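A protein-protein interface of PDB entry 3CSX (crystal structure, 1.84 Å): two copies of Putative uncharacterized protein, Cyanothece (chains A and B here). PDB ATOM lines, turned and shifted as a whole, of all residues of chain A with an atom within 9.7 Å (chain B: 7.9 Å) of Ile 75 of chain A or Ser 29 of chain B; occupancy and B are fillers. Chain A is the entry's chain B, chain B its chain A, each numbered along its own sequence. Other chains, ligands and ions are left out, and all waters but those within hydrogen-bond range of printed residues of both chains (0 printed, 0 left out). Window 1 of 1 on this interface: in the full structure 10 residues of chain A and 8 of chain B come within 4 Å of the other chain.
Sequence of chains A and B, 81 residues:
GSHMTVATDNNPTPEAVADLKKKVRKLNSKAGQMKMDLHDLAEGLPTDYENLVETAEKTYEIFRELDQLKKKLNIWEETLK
OE1 of Glu 78 of chain A is in salt-bridge range of NZ of Lys 21 of chain B (3.2 Å). The guanidinium group of Arg 25 of chain B is in hydrogen-bond range of the side-chain amide oxygen of Asn 11 of chain A, 3.3 Å away. OE1 of Gln 33 of chain B sits at hydrogen-bond distance from NE2 of Gln 68 of chain A, at 3.0 Å. SD of Met 36 of chain B is in hydrogen-bond range of NE2 of Gln 68 of chain A (3.3 Å).
The side-chain hydroxyl (OG) of Ser 29 of chain B is in hydrogen-bond range of the backbone carbonyl oxygen (O) of Arg 25 of chain B, 3.4 Å away. OD1 of Asp 67 of chain A is in salt-bridge range of NZ of Lys 71 of chain A, at 3.1 Å.
Among the printed residues, merely in contact across the chains: Ile 75 of chain A with Asn 28 of chain B (3.1 Å), Asp 67 of chain A with Met 36 of chain B (3.3 Å), Asn 11 of chain A with Lys 22 of chain B (3.5 Å), Ile 75 of chain A with Arg 25 of chain B (3.6 Å), Pro 12 of chain A with Arg 25 of chain B (3.6 Å), Ile 75 of chain A with Ser 29 of chain B (3.7 Å), Lys 71 of chain A with Met 36 of chain B (3.7 Å) and Trp 76 of chain A with Arg 25 of chain B (3.8 Å).
Of the printed residues of chain B, Ile 75 of chain A touches Arg 25 (3.6 Å), Asn 28 (3.1 Å) and Ser 29 (3.7 Å). Ser 29 of chain B touches just one residue of chain A: Ile 75. Ala 31 of chain B touches none of the printed residues of chain A. No residue of chain A comes within 4 Å of Gly 32 of chain B. Printed residues of chain B within 4 Å of Glu 78 of chain A: Lys 21 (3.2 Å). Printed residues of chain B within 4 Å of Trp 76 of chain A: Arg 25. Ile 62 of chain B touches none of the printed residues of chain A. Leu 27 of chain B touches none of the printed residues of chain A. The nearest residue of chain B that does not touch Ile 75 of chain A is Lys 26 of chain B (6.0 Å). The nearest residue of chain A that does not touch Ser 29 of chain B is Lys 72 of chain A (5.8 Å).
Hydrophobic or aromatic side chains of chain A within 4 Å of the printed part of chain B: Pro 12, Ile 75 and Trp 76. Along chain A the printed residues that touch a printed residue of chain B span positions 11 to 78. Among the printed residues, 12 pairs touch across the chains.
No position is printed for both chains.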
ATOM      1  N   ASN A  11      13.728  -7.348   3.026  1.00  0.00           N
ATOM      2  CA  ASN A  11      13.477  -5.922   2.968  1.00  0.00           C
ATOM      3  C   ASN A  11      12.303  -5.534   3.865  1.00  0.00           C
ATOM      4  O   ASN A  11      11.384  -6.341   4.100  1.00  0.00           O
ATOM      5  CB  ASN A  11      13.336  -5.450   1.505  1.00  0.00           C
ATOM      6  CG  ASN A  11      14.541  -5.868   0.631  1.00  0.00           C
ATOM      7  OD1 ASN A  11      15.698  -5.820   1.065  1.00  0.00           O
ATOM      8  ND2 ASN A  11      14.258  -6.313  -0.584  1.00  0.00           N
ATOM      9  N   PRO A  12      12.333  -4.301   4.391  1.00  0.00           N
ATOM     10  CA  PRO A  12      11.294  -3.975   5.355  1.00  0.00           C
ATOM     11  C   PRO A  12       9.911  -3.873   4.703  1.00  0.00           C
ATOM     12  O   PRO A  12       9.780  -3.500   3.540  1.00  0.00           O
ATOM     13  CB  PRO A  12      11.740  -2.625   5.941  1.00  0.00           C
ATOM     14  CG  PRO A  12      13.150  -2.378   5.403  1.00  0.00           C
ATOM     15  CD  PRO A  12      13.235  -3.164   4.126  1.00  0.00           C
ATOM     16  N   THR A  13       8.916  -4.248   5.488  1.00  0.00           N
ATOM     17  CA  THR A  13       7.512  -4.366   5.121  1.00  0.00           C
ATOM     18  C   THR A  13       6.735  -3.403   6.033  1.00  0.00           C
ATOM     19  O   THR A  13       7.262  -3.029   7.091  1.00  0.00           O
ATOM     20  CB  THR A  13       7.075  -5.785   5.476  1.00  0.00           C
ATOM     21  OG1 THR A  13       5.928  -5.734   6.297  1.00  0.00           O
ATOM     22  CG2 THR A  13       8.113  -6.413   6.339  1.00  0.00           C
ATOM     23  N   VAL A  17       7.756  -2.621   9.984  1.00  0.00           N
ATOM     24  CA  VAL A  17       7.838  -1.256  10.496  1.00  0.00           C
ATOM     25  C   VAL A  17       6.937  -1.101  11.726  1.00  0.00           C
ATOM     26  O   VAL A  17       7.379  -0.567  12.744  1.00  0.00           O
ATOM     27  CB  VAL A  17       7.517  -0.190   9.422  1.00  0.00           C
ATOM     28  CG1 VAL A  17       7.404   1.174  10.065  1.00  0.00           C
ATOM     29  CG2 VAL A  17       8.590  -0.174   8.315  1.00  0.00           C
ATOM     30  N   LEU A  20       8.610  -2.687  14.772  1.00  0.00           N
ATOM     31  CA  LEU A  20       9.749  -1.885  15.249  1.00  0.00           C
ATOM     32  C   LEU A  20       9.246  -0.645  15.988  1.00  0.00           C
ATOM     33  O   LEU A  20       9.743  -0.320  17.072  1.00  0.00           O
ATOM     34  CB  LEU A  20      10.655  -1.477  14.072  1.00  0.00           C
ATOM     35  CG  LEU A  20      11.923  -0.649  14.360  1.00  0.00           C
ATOM     36  CD1 LEU A  20      12.813  -1.296  15.426  1.00  0.00           C
ATOM     37  CD2 LEU A  20      12.725  -0.449  13.095  1.00  0.00           C
ATOM     38  N   ASP A  67      18.583   4.620  20.366  1.00  0.00           N
ATOM     39  CA  ASP A  67      19.055   5.471  19.237  1.00  0.00           C
ATOM     40  C   ASP A  67      19.278   4.578  18.012  1.00  0.00           C
ATOM     41  O   ASP A  67      18.854   4.904  16.925  1.00  0.00           O
ATOM     42  CB  ASP A  67      20.362   6.138  19.655  1.00  0.00           C
ATOM     43  CG  ASP A  67      20.852   7.215  18.670  1.00  0.00           C
ATOM     44  OD1 ASP A  67      20.039   7.875  17.994  1.00  0.00           O
ATOM     45  OD2 ASP A  67      22.080   7.381  18.617  1.00  0.00           O
ATOM     46  N   GLN A  68      19.897   3.413  18.204  1.00  0.00           N
ATOM     47  CA  GLN A  68      20.041   2.469  17.084  1.00  0.00           C
ATOM     48  C   GLN A  68      18.718   2.095  16.460  1.00  0.00           C
ATOM     49  O   GLN A  68      18.600   2.020  15.240  1.00  0.00           O
ATOM     50  CB  GLN A  68      20.773   1.168  17.503  1.00  0.00           C
ATOM     51  CG  GLN A  68      22.187   1.390  17.985  1.00  0.00           C
ATOM     52  CD  GLN A  68      23.229   1.468  16.864  1.00  0.00           C
ATOM     53  OE1 GLN A  68      22.896   1.680  15.717  1.00  0.00           O
ATOM     54  NE2 GLN A  68      24.509   1.290  17.221  1.00  0.00           N
ATOM     55  N   LEU A  69      17.702   1.841  17.286  1.00  0.00           N
ATOM     56  CA  LEU A  69      16.448   1.388  16.735  1.00  0.00           C
ATOM     57  C   LEU A  69      15.740   2.537  16.014  1.00  0.00           C
ATOM     58  O   LEU A  69      15.156   2.356  14.944  1.00  0.00           O
ATOM     59  CB  LEU A  69      15.580   0.783  17.833  1.00  0.00           C
ATOM     60  CG  LEU A  69      16.073  -0.543  18.414  1.00  0.00           C
ATOM     61  CD1 LEU A  69      15.159  -0.877  19.609  1.00  0.00           C
ATOM     62  CD2 LEU A  69      16.064  -1.654  17.341  1.00  0.00           C
ATOM     63  N   LYS A  70      15.829   3.725  16.596  1.00  0.00           N
ATOM     64  CA  LYS A  70      15.226   4.891  15.961  1.00  0.00           C
ATOM     65  C   LYS A  70      15.824   5.192  14.589  1.00  0.00           C
ATOM     66  O   LYS A  70      15.096   5.420  13.620  1.00  0.00           O
ATOM     67  CB  LYS A  70      15.259   6.099  16.909  1.00  0.00           C
ATOM     68  CG  LYS A  70      14.137   6.011  17.927  1.00  0.00           C
ATOM     69  CD  LYS A  70      14.151   7.177  18.891  1.00  0.00           C
ATOM     70  CE  LYS A  70      13.183   6.952  20.047  1.00  0.00           C
ATOM     71  NZ  LYS A  70      12.940   8.262  20.735  1.00  0.00           N
ATOM     72  N   LYS A  71      17.146   5.161  14.510  1.00  0.00           N
ATOM     73  CA  LYS A  71      17.876   5.308  13.236  1.00  0.00           C
ATOM     74  C   LYS A  71      17.527   4.201  12.236  1.00  0.00           C
ATOM     75  O   LYS A  71      17.341   4.488  11.062  1.00  0.00           O
ATOM     76  CB  LYS A  71      19.382   5.336  13.491  1.00  0.00           C
ATOM     77  CG  LYS A  71      19.833   6.632  14.187  1.00  0.00           C
ATOM     78  CD  LYS A  71      21.268   6.571  14.736  1.00  0.00           C
ATOM     79  CE  LYS A  71      21.891   7.989  14.815  1.00  0.00           C
ATOM     80  NZ  LYS A  71      20.894   9.043  15.271  1.00  0.00           N
ATOM     81  N   LYS A  72      17.449   2.947  12.708  1.00  0.00           N
ATOM     82  CA  LYS A  72      17.002   1.825  11.871  1.00  0.00           C
ATOM     83  C   LYS A  72      15.598   2.088  11.324  1.00  0.00           C
ATOM     84  O   LYS A  72      15.358   1.918  10.117  1.00  0.00           O
ATOM     85  CB  LYS A  72      17.028   0.484  12.654  1.00  0.00           C
ATOM     86  CG  LYS A  72      16.831  -0.746  11.759  1.00  0.00           C
ATOM     87  CD  LYS A  72      17.130  -2.059  12.467  1.00  0.00           C
ATOM     88  CE  LYS A  72      15.989  -2.489  13.427  1.00  0.00           C
ATOM     89  NZ  LYS A  72      16.407  -3.720  14.151  1.00  0.00           N
ATOM     90  N   LEU A  73      14.684   2.504  12.209  1.00  0.00           N
ATOM     91  CA  LEU A  73      13.290   2.804  11.816  1.00  0.00           C
ATOM     92  C   LEU A  73      13.243   3.830  10.690  1.00  0.00           C
ATOM     93  O   LEU A  73      12.577   3.616   9.667  1.00  0.00           O
ATOM     94  CB  LEU A  73      12.451   3.279  13.008  1.00  0.00           C
ATOM     95  CG  LEU A  73      10.993   3.713  12.725  1.00  0.00           C
ATOM     96  CD1 LEU A  73      10.194   2.563  12.135  1.00  0.00           C
ATOM     97  CD2 LEU A  73      10.320   4.218  13.977  1.00  0.00           C
ATOM     98  N   ASN A  74      13.974   4.921  10.848  1.00  0.00           N
ATOM     99  CA  ASN A  74      14.020   5.929   9.786  1.00  0.00           C
ATOM    100  C   ASN A  74      14.495   5.324   8.473  1.00  0.00           C
ATOM    101  O   ASN A  74      13.852   5.509   7.430  1.00  0.00           O
ATOM    102  CB  ASN A  74      14.881   7.130  10.176  1.00  0.00           C
ATOM    103  CG  ASN A  74      14.213   8.032  11.193  1.00  0.00           C
ATOM    104  OD1 ASN A  74      13.001   8.288  11.125  1.00  0.00           O
ATOM    105  ND2 ASN A  74      15.002   8.535  12.151  1.00  0.00           N
ATOM    106  N   ILE A  75      15.588   4.563   8.530  1.00  0.00           N
ATOM    107  CA  ILE A  75      16.127   3.896   7.336  1.00  0.00           C
ATOM    108  C   ILE A  75      15.107   2.932   6.723  1.00  0.00           C
ATOM    109  O   ILE A  75      14.916   2.931   5.500  1.00  0.00           O
ATOM    110  CB  ILE A  75      17.472   3.181   7.619  1.00  0.00           C
ATOM    111  CG1 ILE A  75      18.624   4.199   7.634  1.00  0.00           C
ATOM    112  CG2 ILE A  75      17.775   2.109   6.571  1.00  0.00           C
ATOM    113  CD1 ILE A  75      19.831   3.766   8.484  1.00  0.00           C
ATOM    114  N   TRP A  76      14.440   2.140   7.564  1.00  0.00           N
ATOM    115  CA  TRP A  76      13.436   1.179   7.101  1.00  0.00           C
ATOM    116  C   TRP A  76      12.282   1.867   6.380  1.00  0.00           C
ATOM    117  O   TRP A  76      11.940   1.511   5.233  1.00  0.00           O
ATOM    118  CB  TRP A  76      12.889   0.369   8.280  1.00  0.00           C
ATOM    119  CG  TRP A  76      13.753  -0.793   8.670  1.00  0.00           C
ATOM    120  CD1 TRP A  76      15.059  -0.998   8.338  1.00  0.00           C
ATOM    121  CD2 TRP A  76      13.366  -1.900   9.500  1.00  0.00           C
ATOM    122  NE1 TRP A  76      15.505  -2.185   8.894  1.00  0.00           N
ATOM    123  CE2 TRP A  76      14.495  -2.741   9.629  1.00  0.00           C
ATOM    124  CE3 TRP A  76      12.172  -2.263  10.141  1.00  0.00           C
ATOM    125  CZ2 TRP A  76      14.461  -3.931  10.360  1.00  0.00           C
ATOM    126  CZ3 TRP A  76      12.142  -3.433  10.879  1.00  0.00           C
ATOM    127  CH2 TRP A  76      13.284  -4.262  10.978  1.00  0.00           C
ATOM    128  N   GLU A  77      11.692   2.851   7.063  1.00  0.00           N
ATOM    129  CA  GLU A  77      10.569   3.625   6.545  1.00  0.00           C
ATOM    130  C   GLU A  77      10.896   4.210   5.177  1.00  0.00           C
ATOM    131  O   GLU A  77      10.056   4.170   4.271  1.00  0.00           O
ATOM    132  CB  GLU A  77      10.164   4.716   7.542  1.00  0.00           C
ATOM    133  CG  GLU A  77       9.421   4.158   8.763  1.00  0.00           C
ATOM    134  CD  GLU A  77       8.777   5.215   9.631  1.00  0.00           C
ATOM    135  OE1 GLU A  77       9.108   6.413   9.507  1.00  0.00           O
ATOM    136  OE2 GLU A  77       7.923   4.839  10.457  1.00  0.00           O
ATOM    137  N   GLU A  78      12.109   4.766   5.073  1.00  0.00           N
ATOM    138  CA  GLU A  78      12.846   5.080   3.828  1.00  0.00           C
ATOM    139  C   GLU A  78      12.387   6.265   2.979  1.00  0.00           C
ATOM    140  O   GLU A  78      12.968   7.360   3.063  1.00  0.00           O
ATOM    141  CB  GLU A  78      13.127   3.825   2.965  1.00  0.00           C
ATOM    142  CG  GLU A  78      11.999   3.315   2.056  1.00  0.00           C
ATOM    143  CD  GLU A  78      12.364   2.017   1.336  1.00  0.00           C
ATOM    144  OE1 GLU A  78      11.438   1.356   0.805  1.00  0.00           O
ATOM    145  OE2 GLU A  78      13.568   1.658   1.296  1.00  0.00           O
ATOM    146  N   LYS B  21      18.262  -0.267  -4.021  1.00  0.00           N
ATOM    147  CA  LYS B  21      17.619   0.214  -2.785  1.00  0.00           C
ATOM    148  C   LYS B  21      18.086  -0.509  -1.519  1.00  0.00           C
ATOM    149  O   LYS B  21      18.300   0.126  -0.480  1.00  0.00           O
ATOM    150  CB  LYS B  21      16.091   0.166  -2.899  1.00  0.00           C
ATOM    151  CG  LYS B  21      15.479   1.442  -3.454  1.00  0.00           C
ATOM    152  CD  LYS B  21      13.970   1.321  -3.614  1.00  0.00           C
ATOM    153  CE  LYS B  21      13.240   1.448  -2.274  1.00  0.00           C
ATOM    154  NZ  LYS B  21      11.951   0.685  -2.282  1.00  0.00           N
ATOM    155  N   LYS B  22      18.242  -1.829  -1.622  1.00  0.00           N
ATOM    156  CA  LYS B  22      18.729  -2.644  -0.521  1.00  0.00           C
ATOM    157  C   LYS B  22      20.195  -2.323  -0.280  1.00  0.00           C
ATOM    158  O   LYS B  22      20.653  -2.319   0.860  1.00  0.00           O
ATOM    159  CB  LYS B  22      18.567  -4.132  -0.842  1.00  0.00           C
ATOM    160  CG  LYS B  22      19.073  -5.088   0.256  1.00  0.00           C
ATOM    161  CD  LYS B  22      19.184  -6.529  -0.244  1.00  0.00           C
ATOM    162  CE  LYS B  22      20.044  -6.634  -1.502  1.00  0.00           C
ATOM    163  NZ  LYS B  22      20.489  -8.037  -1.729  1.00  0.00           N
ATOM    164  N   LYS B  23      20.920  -2.076  -1.368  1.00  0.00           N
ATOM    165  CA  LYS B  23      22.337  -1.762  -1.301  1.00  0.00           C
ATOM    166  C   LYS B  23      22.590  -0.385  -0.682  1.00  0.00           C
ATOM    167  O   LYS B  23      23.536  -0.227   0.080  1.00  0.00           O
ATOM    168  CB  LYS B  23      22.983  -1.876  -2.682  1.00  0.00           C
ATOM    169  CG  LYS B  23      23.091  -3.330  -3.176  1.00  0.00           C
ATOM    170  CD  LYS B  23      24.071  -3.462  -4.343  1.00  0.00           C
ATOM    171  CE  LYS B  23      23.371  -3.323  -5.691  1.00  0.00           C
ATOM    172  NZ  LYS B  23      24.364  -3.187  -6.798  1.00  0.00           N
ATOM    173  N   VAL B  24      21.737   0.583  -1.002  1.00  0.00           N
ATOM    174  CA  VAL B  24      21.770   1.916  -0.386  1.00  0.00           C
ATOM    175  C   VAL B  24      21.368   1.829   1.094  1.00  0.00           C
ATOM    176  O   VAL B  24      21.971   2.456   1.951  1.00  0.00           O
ATOM    177  CB  VAL B  24      20.873   2.907  -1.172  1.00  0.00           C
ATOM    178  CG1 VAL B  24      20.614   4.198  -0.398  1.00  0.00           C
ATOM    179  CG2 VAL B  24      21.498   3.204  -2.525  1.00  0.00           C
ATOM    180  N   ARG B  25      20.349   1.023   1.378  1.00  0.00           N
ATOM    181  CA  ARG B  25      19.908   0.782   2.739  1.00  0.00           C
ATOM    182  C   ARG B  25      21.055   0.239   3.581  1.00  0.00           C
ATOM    183  O   ARG B  25      21.312   0.731   4.686  1.00  0.00           O
ATOM    184  CB  ARG B  25      18.716  -0.175   2.716  1.00  0.00           C
ATOM    185  CG  ARG B  25      18.053  -0.376   4.045  1.00  0.00           C
ATOM    186  CD  ARG B  25      16.662  -0.931   3.841  1.00  0.00           C
ATOM    187  NE  ARG B  25      16.675  -2.344   3.474  1.00  0.00           N
ATOM    188  CZ  ARG B  25      16.913  -3.331   4.334  1.00  0.00           C
ATOM    189  NH1 ARG B  25      17.194  -3.047   5.605  1.00  0.00           N
ATOM    190  NH2 ARG B  25      16.894  -4.599   3.923  1.00  0.00           N
ATOM    191  N   LYS B  26      21.770  -0.748   3.045  1.00  0.00           N
ATOM    192  CA  LYS B  26      22.894  -1.363   3.741  1.00  0.00           C
ATOM    193  C   LYS B  26      24.035  -0.383   4.046  1.00  0.00           C
ATOM    194  O   LYS B  26      24.556  -0.354   5.163  1.00  0.00           O
ATOM    195  CB  LYS B  26      23.423  -2.542   2.940  1.00  0.00           C
ATOM    196  CG  LYS B  26      24.407  -3.395   3.697  1.00  0.00           C
ATOM    197  CD  LYS B  26      24.631  -4.723   2.978  1.00  0.00           C
ATOM    198  CE  LYS B  26      25.241  -5.761   3.904  1.00  0.00           C
ATOM    199  NZ  LYS B  26      24.218  -6.738   4.421  1.00  0.00           N
ATOM    200  N   LEU B  27      24.442   0.386   3.039  1.00  0.00           N
ATOM    201  CA  LEU B  27      25.412   1.451   3.251  1.00  0.00           C
ATOM    202  C   LEU B  27      24.916   2.523   4.213  1.00  0.00           C
ATOM    203  O   LEU B  27      25.685   3.044   5.033  1.00  0.00           O
ATOM    204  CB  LEU B  27      25.769   2.104   1.919  1.00  0.00           C
ATOM    205  CG  LEU B  27      26.790   1.348   1.079  1.00  0.00           C
ATOM    206  CD1 LEU B  27      26.953   2.031  -0.272  1.00  0.00           C
ATOM    207  CD2 LEU B  27      28.108   1.303   1.833  1.00  0.00           C
ATOM    208  N   ASN B  28      23.646   2.879   4.098  1.00  0.00           N
ATOM    209  CA  ASN B  28      23.040   3.844   5.029  1.00  0.00           C
ATOM    210  C   ASN B  28      23.291   3.429   6.457  1.00  0.00           C
ATOM    211  O   ASN B  28      23.692   4.242   7.279  1.00  0.00           O
ATOM    212  CB  ASN B  28      21.541   3.935   4.801  1.00  0.00           C
ATOM    213  CG  ASN B  28      21.055   5.358   4.722  1.00  0.00           C
ATOM    214  OD1 ASN B  28      20.295   5.820   5.594  1.00  0.00           O
ATOM    215  ND2 ASN B  28      21.497   6.078   3.700  1.00  0.00           N
ATOM    216  N   SER B  29      23.022   2.154   6.750  1.00  0.00           N
ATOM    217  CA  SER B  29      23.278   1.614   8.074  1.00  0.00           C
ATOM    218  C   SER B  29      24.747   1.610   8.475  1.00  0.00           C
ATOM    219  O   SER B  29      25.066   2.034   9.591  1.00  0.00           O
ATOM    220  CB  SER B  29      22.633   0.227   8.261  1.00  0.00           C
ATOM    221  OG  SER B  29      21.232   0.364   8.108  1.00  0.00           O
ATOM    222  N   LYS B  30      25.627   1.145   7.583  1.00  0.00           N
ATOM    223  CA  LYS B  30      27.063   1.145   7.817  1.00  0.00           C
ATOM    224  C   LYS B  30      27.543   2.590   8.099  1.00  0.00           C
ATOM    225  O   LYS B  30      28.346   2.817   8.983  1.00  0.00           O
ATOM    226  CB  LYS B  30      27.802   0.570   6.602  1.00  0.00           C
ATOM    227  CG  LYS B  30      29.320   0.544   6.716  1.00  0.00           C
ATOM    228  CD  LYS B  30      29.839  -0.668   7.465  1.00  0.00           C
ATOM    229  CE  LYS B  30      31.307  -0.480   7.870  1.00  0.00           C
ATOM    230  NZ  LYS B  30      31.641  -1.375   9.046  1.00  0.00           N
ATOM    231  N   ALA B  31      27.000   3.538   7.346  1.00  0.00           N
ATOM    232  CA  ALA B  31      27.405   4.960   7.438  1.00  0.00           C
ATOM    233  C   ALA B  31      27.009   5.455   8.829  1.00  0.00           C
ATOM    234  O   ALA B  31      27.803   6.086   9.519  1.00  0.00           O
ATOM    235  CB  ALA B  31      26.709   5.764   6.349  1.00  0.00           C
ATOM    236  N   GLY B  32      25.790   5.114   9.261  1.00  0.00           N
ATOM    237  CA  GLY B  32      25.299   5.557  10.567  1.00  0.00           C
ATOM    238  C   GLY B  32      26.150   5.002  11.690  1.00  0.00           C
ATOM    239  O   GLY B  32      26.412   5.681  12.684  1.00  0.00           O
ATOM    240  N   GLN B  33      26.582   3.749  11.535  1.00  0.00           N
ATOM    241  CA  GLN B  33      27.441   3.141  12.550  1.00  0.00           C
ATOM    242  C   GLN B  33      28.833   3.728  12.604  1.00  0.00           C
ATOM    243  O   GLN B  33      29.416   3.829  13.678  1.00  0.00           O
ATOM    244  CB  GLN B  33      27.566   1.623  12.389  1.00  0.00           C
ATOM    245  CG  GLN B  33      28.353   1.010  13.533  1.00  0.00           C
ATOM    246  CD  GLN B  33      27.605   1.124  14.837  1.00  0.00           C
ATOM    247  OE1 GLN B  33      26.419   0.775  14.914  1.00  0.00           O
ATOM    248  NE2 GLN B  33      28.279   1.634  15.871  1.00  0.00           N
ATOM    249  N   MET B  34      29.391   4.072  11.447  1.00  0.00           N
ATOM    250  CA  MET B  34      30.740   4.646  11.441  1.00  0.00           C
ATOM    251  C   MET B  34      30.679   6.076  11.979  1.00  0.00           C
ATOM    252  O   MET B  34      31.598   6.534  12.657  1.00  0.00           O
ATOM    253  CB  MET B  34      31.324   4.618  10.035  1.00  0.00           C
ATOM    254  CG  MET B  34      31.598   3.226   9.462  1.00  0.00           C
ATOM    255  SD  MET B  34      32.749   2.253  10.427  1.00  0.00           S
ATOM    256  CE  MET B  34      34.114   3.417  10.529  1.00  0.00           C
ATOM    257  N   LYS B  35      29.602   6.783  11.655  1.00  0.00           N
ATOM    258  CA  LYS B  35      29.363   8.093  12.281  1.00  0.00           C
ATOM    259  C   LYS B  35      29.393   7.995  13.813  1.00  0.00           C
ATOM    260  O   LYS B  35      30.141   8.713  14.486  1.00  0.00           O
ATOM    261  CB  LYS B  35      28.046   8.685  11.799  1.00  0.00           C
ATOM    262  CG  LYS B  35      27.681  10.018  12.531  1.00  0.00           C
ATOM    263  CD  LYS B  35      26.545  10.707  11.759  1.00  0.00           C
ATOM    264  CE  LYS B  35      26.119  12.032  12.437  1.00  0.00           C
ATOM    265  NZ  LYS B  35      24.926  12.557  11.695  1.00  0.00           N
ATOM    266  N   MET B  36      28.578   7.106  14.376  1.00  0.00           N
ATOM    267  CA  MET B  36      28.597   6.878  15.810  1.00  0.00           C
ATOM    268  C   MET B  36      30.001   6.537  16.318  1.00  0.00           C
ATOM    269  O   MET B  36      30.451   7.043  17.341  1.00  0.00           O
ATOM    270  CB  MET B  36      27.676   5.703  16.179  1.00  0.00           C
ATOM    271  CG  MET B  36      26.219   5.972  16.145  1.00  0.00           C
ATOM    272  SD  MET B  36      25.321   4.389  16.480  1.00  0.00           S
ATOM    273  CE  MET B  36      23.795   5.089  17.055  1.00  0.00           C
ATOM    274  N   ILE B  62      32.930   4.776   3.385  1.00  0.00           N
ATOM    275  CA  ILE B  62      31.530   4.394   3.419  1.00  0.00           C
ATOM    276  C   ILE B  62      30.653   5.587   2.992  1.00  0.00           C
ATOM    277  O   ILE B  62      29.763   5.434   2.145  1.00  0.00           O
ATOM    278  CB  ILE B  62      31.192   3.819   4.806  1.00  0.00           C
ATOM    279  CG1 ILE B  62      31.902   2.455   5.014  1.00  0.00           C
ATOM    280  CG2 ILE B  62      29.694   3.679   5.050  1.00  0.00           C
ATOM    281  CD1 ILE B  62      31.572   1.374   3.957  1.00  0.00           C
ATOM    282  N   LEU B  66      28.301   5.635  -0.280  1.00  0.00           N
ATOM    283  CA  LEU B  66      26.860   5.897  -0.079  1.00  0.00           C
ATOM    284  C   LEU B  66      26.394   7.070  -0.915  1.00  0.00           C
ATOM    285  O   LEU B  66      25.333   7.020  -1.521  1.00  0.00           O
ATOM    286  CB  LEU B  66      26.541   6.172   1.397  1.00  0.00           C
ATOM    287  CG  LEU B  66      25.132   6.645   1.795  1.00  0.00           C
ATOM    288  CD1 LEU B  66      23.982   5.722   1.318  1.00  0.00           C
ATOM    289  CD2 LEU B  66      25.061   6.899   3.301  1.00  0.00           C
